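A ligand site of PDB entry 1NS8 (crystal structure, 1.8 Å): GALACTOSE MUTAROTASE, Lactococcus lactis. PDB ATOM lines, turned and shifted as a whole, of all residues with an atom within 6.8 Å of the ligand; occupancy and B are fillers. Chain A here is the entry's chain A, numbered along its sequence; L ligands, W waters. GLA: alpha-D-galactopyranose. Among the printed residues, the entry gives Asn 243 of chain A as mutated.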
ATOM      1  N   ASP A  58      -5.935 -16.237  34.043  1.00  0.00           N
ATOM      2  CA  ASP A  58      -5.483 -17.045  32.935  1.00  0.00           C
ATOM      3  C   ASP A  58      -4.041 -17.321  33.219  1.00  0.00           C
ATOM      4  O   ASP A  58      -3.295 -16.375  33.360  1.00  0.00           O
ATOM      5  CB  ASP A  58      -5.743 -16.393  31.558  1.00  0.00           C
ATOM      6  CG  ASP A  58      -5.194 -17.257  30.445  1.00  0.00           C
ATOM      7  OD1 ASP A  58      -4.674 -18.338  30.638  1.00  0.00           O
ATOM      8  OD2 ASP A  58      -5.360 -16.748  29.258  1.00  0.00           O
ATOM      9  N   TYR A  60      -1.851 -19.040  31.386  1.00  0.00           N
ATOM     10  CA  TYR A  60      -0.920 -19.218  30.280  1.00  0.00           C
ATOM     11  C   TYR A  60      -0.085 -18.023  29.824  1.00  0.00           C
ATOM     12  O   TYR A  60       1.069 -18.189  29.380  1.00  0.00           O
ATOM     13  CB  TYR A  60      -1.679 -19.797  29.074  1.00  0.00           C
ATOM     14  CG  TYR A  60      -2.167 -21.211  29.326  1.00  0.00           C
ATOM     15  CD1 TYR A  60      -3.525 -21.516  29.286  1.00  0.00           C
ATOM     16  CD2 TYR A  60      -1.273 -22.262  29.554  1.00  0.00           C
ATOM     17  CE1 TYR A  60      -3.990 -22.805  29.499  1.00  0.00           C
ATOM     18  CE2 TYR A  60      -1.717 -23.567  29.782  1.00  0.00           C
ATOM     19  CZ  TYR A  60      -3.083 -23.839  29.740  1.00  0.00           C
ATOM     20  OH  TYR A  60      -3.542 -25.110  29.921  1.00  0.00           O
ATOM     21  N   PRO A  61      -0.674 -16.822  29.902  1.00  0.00           N
ATOM     22  CA  PRO A  61       0.067 -15.651  29.442  1.00  0.00           C
ATOM     23  C   PRO A  61       1.508 -15.521  29.923  1.00  0.00           C
ATOM     24  O   PRO A  61       1.749 -15.408  31.128  1.00  0.00           O
ATOM     25  CB  PRO A  61      -0.792 -14.417  29.771  1.00  0.00           C
ATOM     26  CG  PRO A  61      -2.198 -14.944  30.018  1.00  0.00           C
ATOM     27  CD  PRO A  61      -2.053 -16.433  30.312  1.00  0.00           C
ATOM     28  N   GLY A  70       0.693 -27.350  23.173  1.00  0.00           N
ATOM     29  CA  GLY A  70      -0.352 -27.630  22.202  1.00  0.00           C
ATOM     30  C   GLY A  70      -1.288 -28.749  22.633  1.00  0.00           C
ATOM     31  O   GLY A  70      -1.256 -29.216  23.794  1.00  0.00           O
ATOM     32  N   ARG A  71      -2.119 -29.151  21.653  1.00  0.00           N
ATOM     33  CA  ARG A  71      -3.082 -30.206  21.837  1.00  0.00           C
ATOM     34  C   ARG A  71      -2.654 -31.536  21.280  1.00  0.00           C
ATOM     35  O   ARG A  71      -2.248 -31.629  20.106  1.00  0.00           O
ATOM     36  CB  ARG A  71      -4.369 -29.911  21.079  1.00  0.00           C
ATOM     37  CG  ARG A  71      -5.012 -28.682  21.613  1.00  0.00           C
ATOM     38  CD  ARG A  71      -6.289 -28.262  20.864  1.00  0.00           C
ATOM     39  NE  ARG A  71      -6.921 -27.238  21.721  1.00  0.00           N
ATOM     40  CZ  ARG A  71      -6.618 -25.951  21.752  1.00  0.00           C
ATOM     41  NH1 ARG A  71      -5.730 -25.386  20.889  1.00  0.00           N
ATOM     42  NH2 ARG A  71      -7.263 -25.211  22.639  1.00  0.00           N
ATOM     43  N   GLU A  90      -8.764 -31.067  28.391  1.00  0.00           N
ATOM     44  CA  GLU A  90      -9.550 -30.285  27.461  1.00  0.00           C
ATOM     45  C   GLU A  90     -10.308 -31.328  26.686  1.00  0.00           C
ATOM     46  O   GLU A  90      -9.921 -31.705  25.565  1.00  0.00           O
ATOM     47  CB  GLU A  90      -8.670 -29.502  26.524  1.00  0.00           C
ATOM     48  CG  GLU A  90      -9.539 -28.488  25.795  1.00  0.00           C
ATOM     49  CD  GLU A  90      -8.912 -27.967  24.546  1.00  0.00           C
ATOM     50  OE1 GLU A  90      -8.418 -28.694  23.717  1.00  0.00           O
ATOM     51  OE2 GLU A  90      -8.941 -26.656  24.465  1.00  0.00           O
ATOM     52  N   LEU A  95      -4.000 -30.729  26.619  1.00  0.00           N
ATOM     53  CA  LEU A  95      -3.599 -29.412  26.127  1.00  0.00           C
ATOM     54  C   LEU A  95      -2.515 -28.823  27.030  1.00  0.00           C
ATOM     55  O   LEU A  95      -2.689 -28.778  28.213  1.00  0.00           O
ATOM     56  CB  LEU A  95      -4.807 -28.432  26.115  1.00  0.00           C
ATOM     57  CG  LEU A  95      -4.377 -26.964  25.984  1.00  0.00           C
ATOM     58  CD1 LEU A  95      -4.069 -26.564  24.519  1.00  0.00           C
ATOM     59  CD2 LEU A  95      -5.452 -26.091  26.563  1.00  0.00           C
ATOM     60  N   HIS A  96      -1.412 -28.357  26.458  1.00  0.00           N
ATOM     61  CA  HIS A  96      -0.316 -27.764  27.245  1.00  0.00           C
ATOM     62  C   HIS A  96       0.202 -28.564  28.459  1.00  0.00           C
ATOM     63  O   HIS A  96       0.463 -28.018  29.555  1.00  0.00           O
ATOM     64  CB  HIS A  96      -0.636 -26.326  27.677  1.00  0.00           C
ATOM     65  CG  HIS A  96      -0.911 -25.407  26.528  1.00  0.00           C
ATOM     66  ND1 HIS A  96      -0.254 -25.566  25.300  1.00  0.00           N
ATOM     67  CD2 HIS A  96      -1.783 -24.390  26.444  1.00  0.00           C
ATOM     68  CE1 HIS A  96      -0.741 -24.627  24.518  1.00  0.00           C
ATOM     69  NE2 HIS A  96      -1.661 -23.898  25.164  1.00  0.00           N
ATOM     70  N   HIS A 170       4.679 -18.777  26.001  1.00  0.00           N
ATOM     71  CA  HIS A 170       3.353 -18.315  25.666  1.00  0.00           C
ATOM     72  C   HIS A 170       3.066 -16.802  25.846  1.00  0.00           C
ATOM     73  O   HIS A 170       1.973 -16.416  26.268  1.00  0.00           O
ATOM     74  CB  HIS A 170       2.324 -19.122  26.455  1.00  0.00           C
ATOM     75  CG  HIS A 170       1.029 -19.293  25.707  1.00  0.00           C
ATOM     76  ND1 HIS A 170       0.078 -18.271  25.637  1.00  0.00           N
ATOM     77  CD2 HIS A 170       0.565 -20.360  24.996  1.00  0.00           C
ATOM     78  CE1 HIS A 170      -0.928 -18.737  24.909  1.00  0.00           C
ATOM     79  NE2 HIS A 170      -0.672 -19.988  24.506  1.00  0.00           N
ATOM     80  N   TYR A 172       2.103 -13.049  24.877  1.00  0.00           N
ATOM     81  CA  TYR A 172       1.161 -12.388  23.975  1.00  0.00           C
ATOM     82  C   TYR A 172       1.665 -10.946  23.808  1.00  0.00           C
ATOM     83  O   TYR A 172       1.877 -10.185  24.772  1.00  0.00           O
ATOM     84  CB  TYR A 172      -0.214 -12.214  24.614  1.00  0.00           C
ATOM     85  CG  TYR A 172      -1.098 -13.444  24.673  1.00  0.00           C
ATOM     86  CD1 TYR A 172      -1.150 -14.237  25.818  1.00  0.00           C
ATOM     87  CD2 TYR A 172      -1.949 -13.775  23.608  1.00  0.00           C
ATOM     88  CE1 TYR A 172      -1.993 -15.350  25.894  1.00  0.00           C
ATOM     89  CE2 TYR A 172      -2.785 -14.887  23.660  1.00  0.00           C
ATOM     90  CZ  TYR A 172      -2.817 -15.668  24.807  1.00  0.00           C
ATOM     91  OH  TYR A 172      -3.659 -16.781  24.883  1.00  0.00           O
ATOM     92  N   LEU A 198      -6.877 -27.029  11.083  1.00  0.00           N
ATOM     93  CA  LEU A 198      -7.496 -27.698  12.196  1.00  0.00           C
ATOM     94  C   LEU A 198      -8.729 -28.495  11.762  1.00  0.00           C
ATOM     95  O   LEU A 198      -9.462 -28.100  10.872  1.00  0.00           O
ATOM     96  CB  LEU A 198      -7.886 -26.697  13.294  1.00  0.00           C
ATOM     97  CG  LEU A 198      -6.750 -25.752  13.693  1.00  0.00           C
ATOM     98  CD1 LEU A 198      -7.172 -25.001  14.943  1.00  0.00           C
ATOM     99  CD2 LEU A 198      -5.465 -26.537  13.969  1.00  0.00           C
ATOM    100  N   GLU A 203     -10.153 -28.260  17.762  1.00  0.00           N
ATOM    101  CA  GLU A 203      -8.861 -27.731  17.448  1.00  0.00           C
ATOM    102  C   GLU A 203      -7.775 -28.754  17.291  1.00  0.00           C
ATOM    103  O   GLU A 203      -6.606 -28.441  17.354  1.00  0.00           O
ATOM    104  CB  GLU A 203      -8.470 -26.540  18.340  1.00  0.00           C
ATOM    105  CG  GLU A 203      -9.416 -25.308  18.152  1.00  0.00           C
ATOM    106  CD  GLU A 203      -9.690 -24.431  19.383  1.00  0.00           C
ATOM    107  OE1 GLU A 203     -10.747 -24.393  20.032  1.00  0.00           O
ATOM    108  OE2 GLU A 203      -8.665 -23.682  19.691  1.00  0.00           O
ATOM    109  N   ASN A 243      -5.204 -19.396  14.846  1.00  0.00           N
ATOM    110  CA  ASN A 243      -4.863 -20.339  15.914  1.00  0.00           C
ATOM    111  C   ASN A 243      -4.293 -21.535  15.236  1.00  0.00           C
ATOM    112  O   ASN A 243      -4.904 -22.574  15.277  1.00  0.00           O
ATOM    113  CB  ASN A 243      -6.124 -20.756  16.674  1.00  0.00           C
ATOM    114  CG  ASN A 243      -5.734 -21.327  18.011  1.00  0.00           C
ATOM    115  OD1 ASN A 243      -4.547 -21.463  18.294  1.00  0.00           O
ATOM    116  ND2 ASN A 243      -6.727 -21.626  18.809  1.00  0.00           N
ATOM    117  N   HIS A 244      -3.122 -21.366  14.583  1.00  0.00           N
ATOM    118  CA  HIS A 244      -2.543 -22.410  13.779  1.00  0.00           C
ATOM    119  C   HIS A 244      -1.054 -22.390  13.743  1.00  0.00           C
ATOM    120  O   HIS A 244      -0.428 -21.343  13.918  1.00  0.00           O
ATOM    121  CB  HIS A 244      -2.871 -22.085  12.306  1.00  0.00           C
ATOM    122  CG  HIS A 244      -4.337 -22.153  12.014  1.00  0.00           C
ATOM    123  ND1 HIS A 244      -5.241 -21.143  12.407  1.00  0.00           N
ATOM    124  CD2 HIS A 244      -5.017 -23.135  11.375  1.00  0.00           C
ATOM    125  CE1 HIS A 244      -6.440 -21.545  12.022  1.00  0.00           C
ATOM    126  NE2 HIS A 244      -6.340 -22.726  11.386  1.00  0.00           N
ATOM    127  N   VAL A 277       3.357 -21.439  16.220  1.00  0.00           N
ATOM    128  CA  VAL A 277       1.926 -21.458  16.355  1.00  0.00           C
ATOM    129  C   VAL A 277       1.496 -20.028  16.623  1.00  0.00           C
ATOM    130  O   VAL A 277       2.046 -19.379  17.526  1.00  0.00           O
ATOM    131  CB  VAL A 277       1.461 -22.351  17.505  1.00  0.00           C
ATOM    132  CG1 VAL A 277      -0.051 -22.084  17.717  1.00  0.00           C
ATOM    133  CG2 VAL A 277       1.676 -23.824  17.121  1.00  0.00           C
ATOM    134  N   ILE A 278       0.545 -19.518  15.847  1.00  0.00           N
ATOM    135  CA  ILE A 278       0.099 -18.134  16.038  1.00  0.00           C
ATOM    136  C   ILE A 278      -1.322 -18.090  16.511  1.00  0.00           C
ATOM    137  O   ILE A 278      -2.201 -18.616  15.840  1.00  0.00           O
ATOM    138  CB  ILE A 278       0.251 -17.308  14.746  1.00  0.00           C
ATOM    139  CG1 ILE A 278       1.739 -17.267  14.390  1.00  0.00           C
ATOM    140  CG2 ILE A 278      -0.287 -15.871  14.910  1.00  0.00           C
ATOM    141  CD1 ILE A 278       2.042 -16.344  13.236  1.00  0.00           C
ATOM    142  N   PHE A 279      -1.524 -17.494  17.676  1.00  0.00           N
ATOM    143  CA  PHE A 279      -2.884 -17.425  18.203  1.00  0.00           C
ATOM    144  C   PHE A 279      -3.199 -15.968  18.480  1.00  0.00           C
ATOM    145  O   PHE A 279      -2.466 -15.284  19.187  1.00  0.00           O
ATOM    146  CB  PHE A 279      -2.964 -18.318  19.466  1.00  0.00           C
ATOM    147  CG  PHE A 279      -4.219 -18.191  20.292  1.00  0.00           C
ATOM    148  CD1 PHE A 279      -5.460 -18.485  19.733  1.00  0.00           C
ATOM    149  CD2 PHE A 279      -4.119 -17.758  21.626  1.00  0.00           C
ATOM    150  CE1 PHE A 279      -6.626 -18.394  20.502  1.00  0.00           C
ATOM    151  CE2 PHE A 279      -5.271 -17.632  22.398  1.00  0.00           C
ATOM    152  CZ  PHE A 279      -6.508 -17.966  21.824  1.00  0.00           C
ATOM    153  N   PHE A 283     -10.719 -14.592  21.989  1.00  0.00           N
ATOM    154  CA  PHE A 283     -11.580 -14.793  23.173  1.00  0.00           C
ATOM    155  C   PHE A 283     -13.010 -14.246  23.155  1.00  0.00           C
ATOM    156  O   PHE A 283     -13.711 -14.269  24.195  1.00  0.00           O
ATOM    157  CB  PHE A 283     -10.887 -14.325  24.452  1.00  0.00           C
ATOM    158  CG  PHE A 283      -9.565 -15.007  24.664  1.00  0.00           C
ATOM    159  CD1 PHE A 283      -8.362 -14.287  24.705  1.00  0.00           C
ATOM    160  CD2 PHE A 283      -9.513 -16.390  24.851  1.00  0.00           C
ATOM    161  CE1 PHE A 283      -7.157 -14.948  24.941  1.00  0.00           C
ATOM    162  CE2 PHE A 283      -8.309 -17.064  25.083  1.00  0.00           C
ATOM    163  CZ  PHE A 283      -7.126 -16.325  25.119  1.00  0.00           C
ATOM    164  N   THR A 302       0.302 -14.371  19.823  1.00  0.00           N
ATOM    165  CA  THR A 302       1.434 -15.156  20.274  1.00  0.00           C
ATOM    166  C   THR A 302       2.298 -15.588  19.117  1.00  0.00           C
ATOM    167  O   THR A 302       1.851 -15.608  17.978  1.00  0.00           O
ATOM    168  CB  THR A 302       0.932 -16.493  20.895  1.00  0.00           C
ATOM    169  OG1 THR A 302       0.302 -17.303  19.880  1.00  0.00           O
ATOM    170  CG2 THR A 302       0.019 -16.342  22.110  1.00  0.00           C
ATOM    171  N   GLU A 304       4.251 -18.906  19.273  1.00  0.00           N
ATOM    172  CA  GLU A 304       4.654 -20.114  19.969  1.00  0.00           C
ATOM    173  C   GLU A 304       5.570 -20.955  19.096  1.00  0.00           C
ATOM    174  O   GLU A 304       5.150 -21.700  18.221  1.00  0.00           O
ATOM    175  CB  GLU A 304       3.471 -20.903  20.556  1.00  0.00           C
ATOM    176  CG  GLU A 304       2.530 -19.981  21.365  1.00  0.00           C
ATOM    177  CD  GLU A 304       1.129 -20.539  21.591  1.00  0.00           C
ATOM    178  OE1 GLU A 304       0.895 -21.597  22.123  1.00  0.00           O
ATOM    179  OE2 GLU A 304       0.175 -19.760  21.174  1.00  0.00           O
HETATM  180  C1  GLA L   1      -2.576 -22.002  22.367  1.00  0.00           C
HETATM  181  C2  GLA L   1      -3.867 -22.568  21.740  1.00  0.00           C
HETATM  182  C3  GLA L   1      -5.065 -21.702  22.012  1.00  0.00           C
HETATM  183  C4  GLA L   1      -5.202 -21.420  23.505  1.00  0.00           C
HETATM  184  C5  GLA L   1      -3.872 -20.900  24.078  1.00  0.00           C
HETATM  185  C6  GLA L   1      -3.851 -20.755  25.601  1.00  0.00           C
HETATM  186  O1  GLA L   1      -2.227 -20.749  21.781  1.00  0.00           O
HETATM  187  O2  GLA L   1      -3.824 -22.811  20.337  1.00  0.00           O
HETATM  188  O3  GLA L   1      -6.223 -22.442  21.581  1.00  0.00           O
HETATM  189  O4  GLA L   1      -5.683 -22.547  24.228  1.00  0.00           O
HETATM  190  O5  GLA L   1      -2.782 -21.779  23.778  1.00  0.00           O
HETATM  191  O6  GLA L   1      -5.105 -20.224  26.034  1.00  0.00           O
HETATM  192  O   HOH W   1      -4.020 -17.761  27.354  1.00  0.00           O
HETATM  193  O   HOH W   2      -3.555 -24.362  17.227  1.00  0.00           O
HETATM  194  O   HOH W   3      -8.703 -21.166  21.744  1.00  0.00           O
HETATM  195  O   HOH W   4      -1.601 -24.789  20.128  1.00  0.00           O
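Water W3 bridges an oxygen (O3) of the ligand and the side-chain carboxylate (OE2) of Glu 203.
Water W1 lies within hydrogen-bond range of OD2 of Asp 58 (2.5 Å), OH of Tyr 172 (2.7 Å) and O6 of the ligand (3.0 Å).
Water W2 bridges the backbone carbonyl oxygen of Asn 243 and an oxygen (O2) of the ligand.
NE2 of His 96 is in hydrogen-bond range of O5 of the ligand (2.8 Å).
OE2 of Glu 304 sits at hydrogen-bond distance from O1 of the ligand (2.7 Å).
An oxygen (O3) of the ligand is in hydrogen-bond range of the side-chain carboxylate of Glu 203, at 3.3 Å.
An oxygen (O5) of the ligand sits at hydrogen-bond distance from a ring nitrogen (NE2) of His 170.
An oxygen (O3) of the ligand sits at hydrogen-bond distance from the guanidinium group of Arg 71 (3.1 Å).
The side-chain amide oxygen of Asn 243 lies within hydrogen-bond range of an oxygen (O2) of the ligand (2.6 Å).
The side-chain carboxylate (OE2) of Glu 203 lies within salt-bridge range of the guanidinium group (NH1) of Arg 71, at 3.6 Å.
The side-chain carboxylate of Glu 304 sits close to a ring nitrogen (NE2) of His 170 (3.3 Å).
OG1 of Thr 302 sits at hydrogen-bond distance from N of Phe 279 (2.9 Å).
The guanidinium group (NH2) of Arg 71 lies within salt-bridge range of the side-chain carboxylate (OE2) of Glu 90.
N of His 96 is in hydrogen-bond range of O of Gly 70.
The side-chain amide nitrogen (ND2) of Asn 243 sits at hydrogen-bond distance from the side-chain carboxylate (OE2) of Glu 203 (3.0 Å).
N of Asn 243 lies close to O of Ile 278, at 3.3 Å.
The backbone NH (N) of Val 277 lies within hydrogen-bond range of the backbone carbonyl oxygen (O) of Glu 304 (2.7 Å).
CD1 of Tyr 60 touches C6 of the ligand, 3.8 Å away.
Tyr 172 touches the ligand.
CB of Phe 279 touches O1 of the ligand, at 3.4 Å.
Hydrophobic or aromatic side chains that line the ligand: Tyr 60, His 96, His 170 and Phe 279.
Of the 20 residues printed, 9 come within 4 Å of the ligand.
The nearest printed residue that does not touch the ligand is Leu 95 (4.3 Å).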
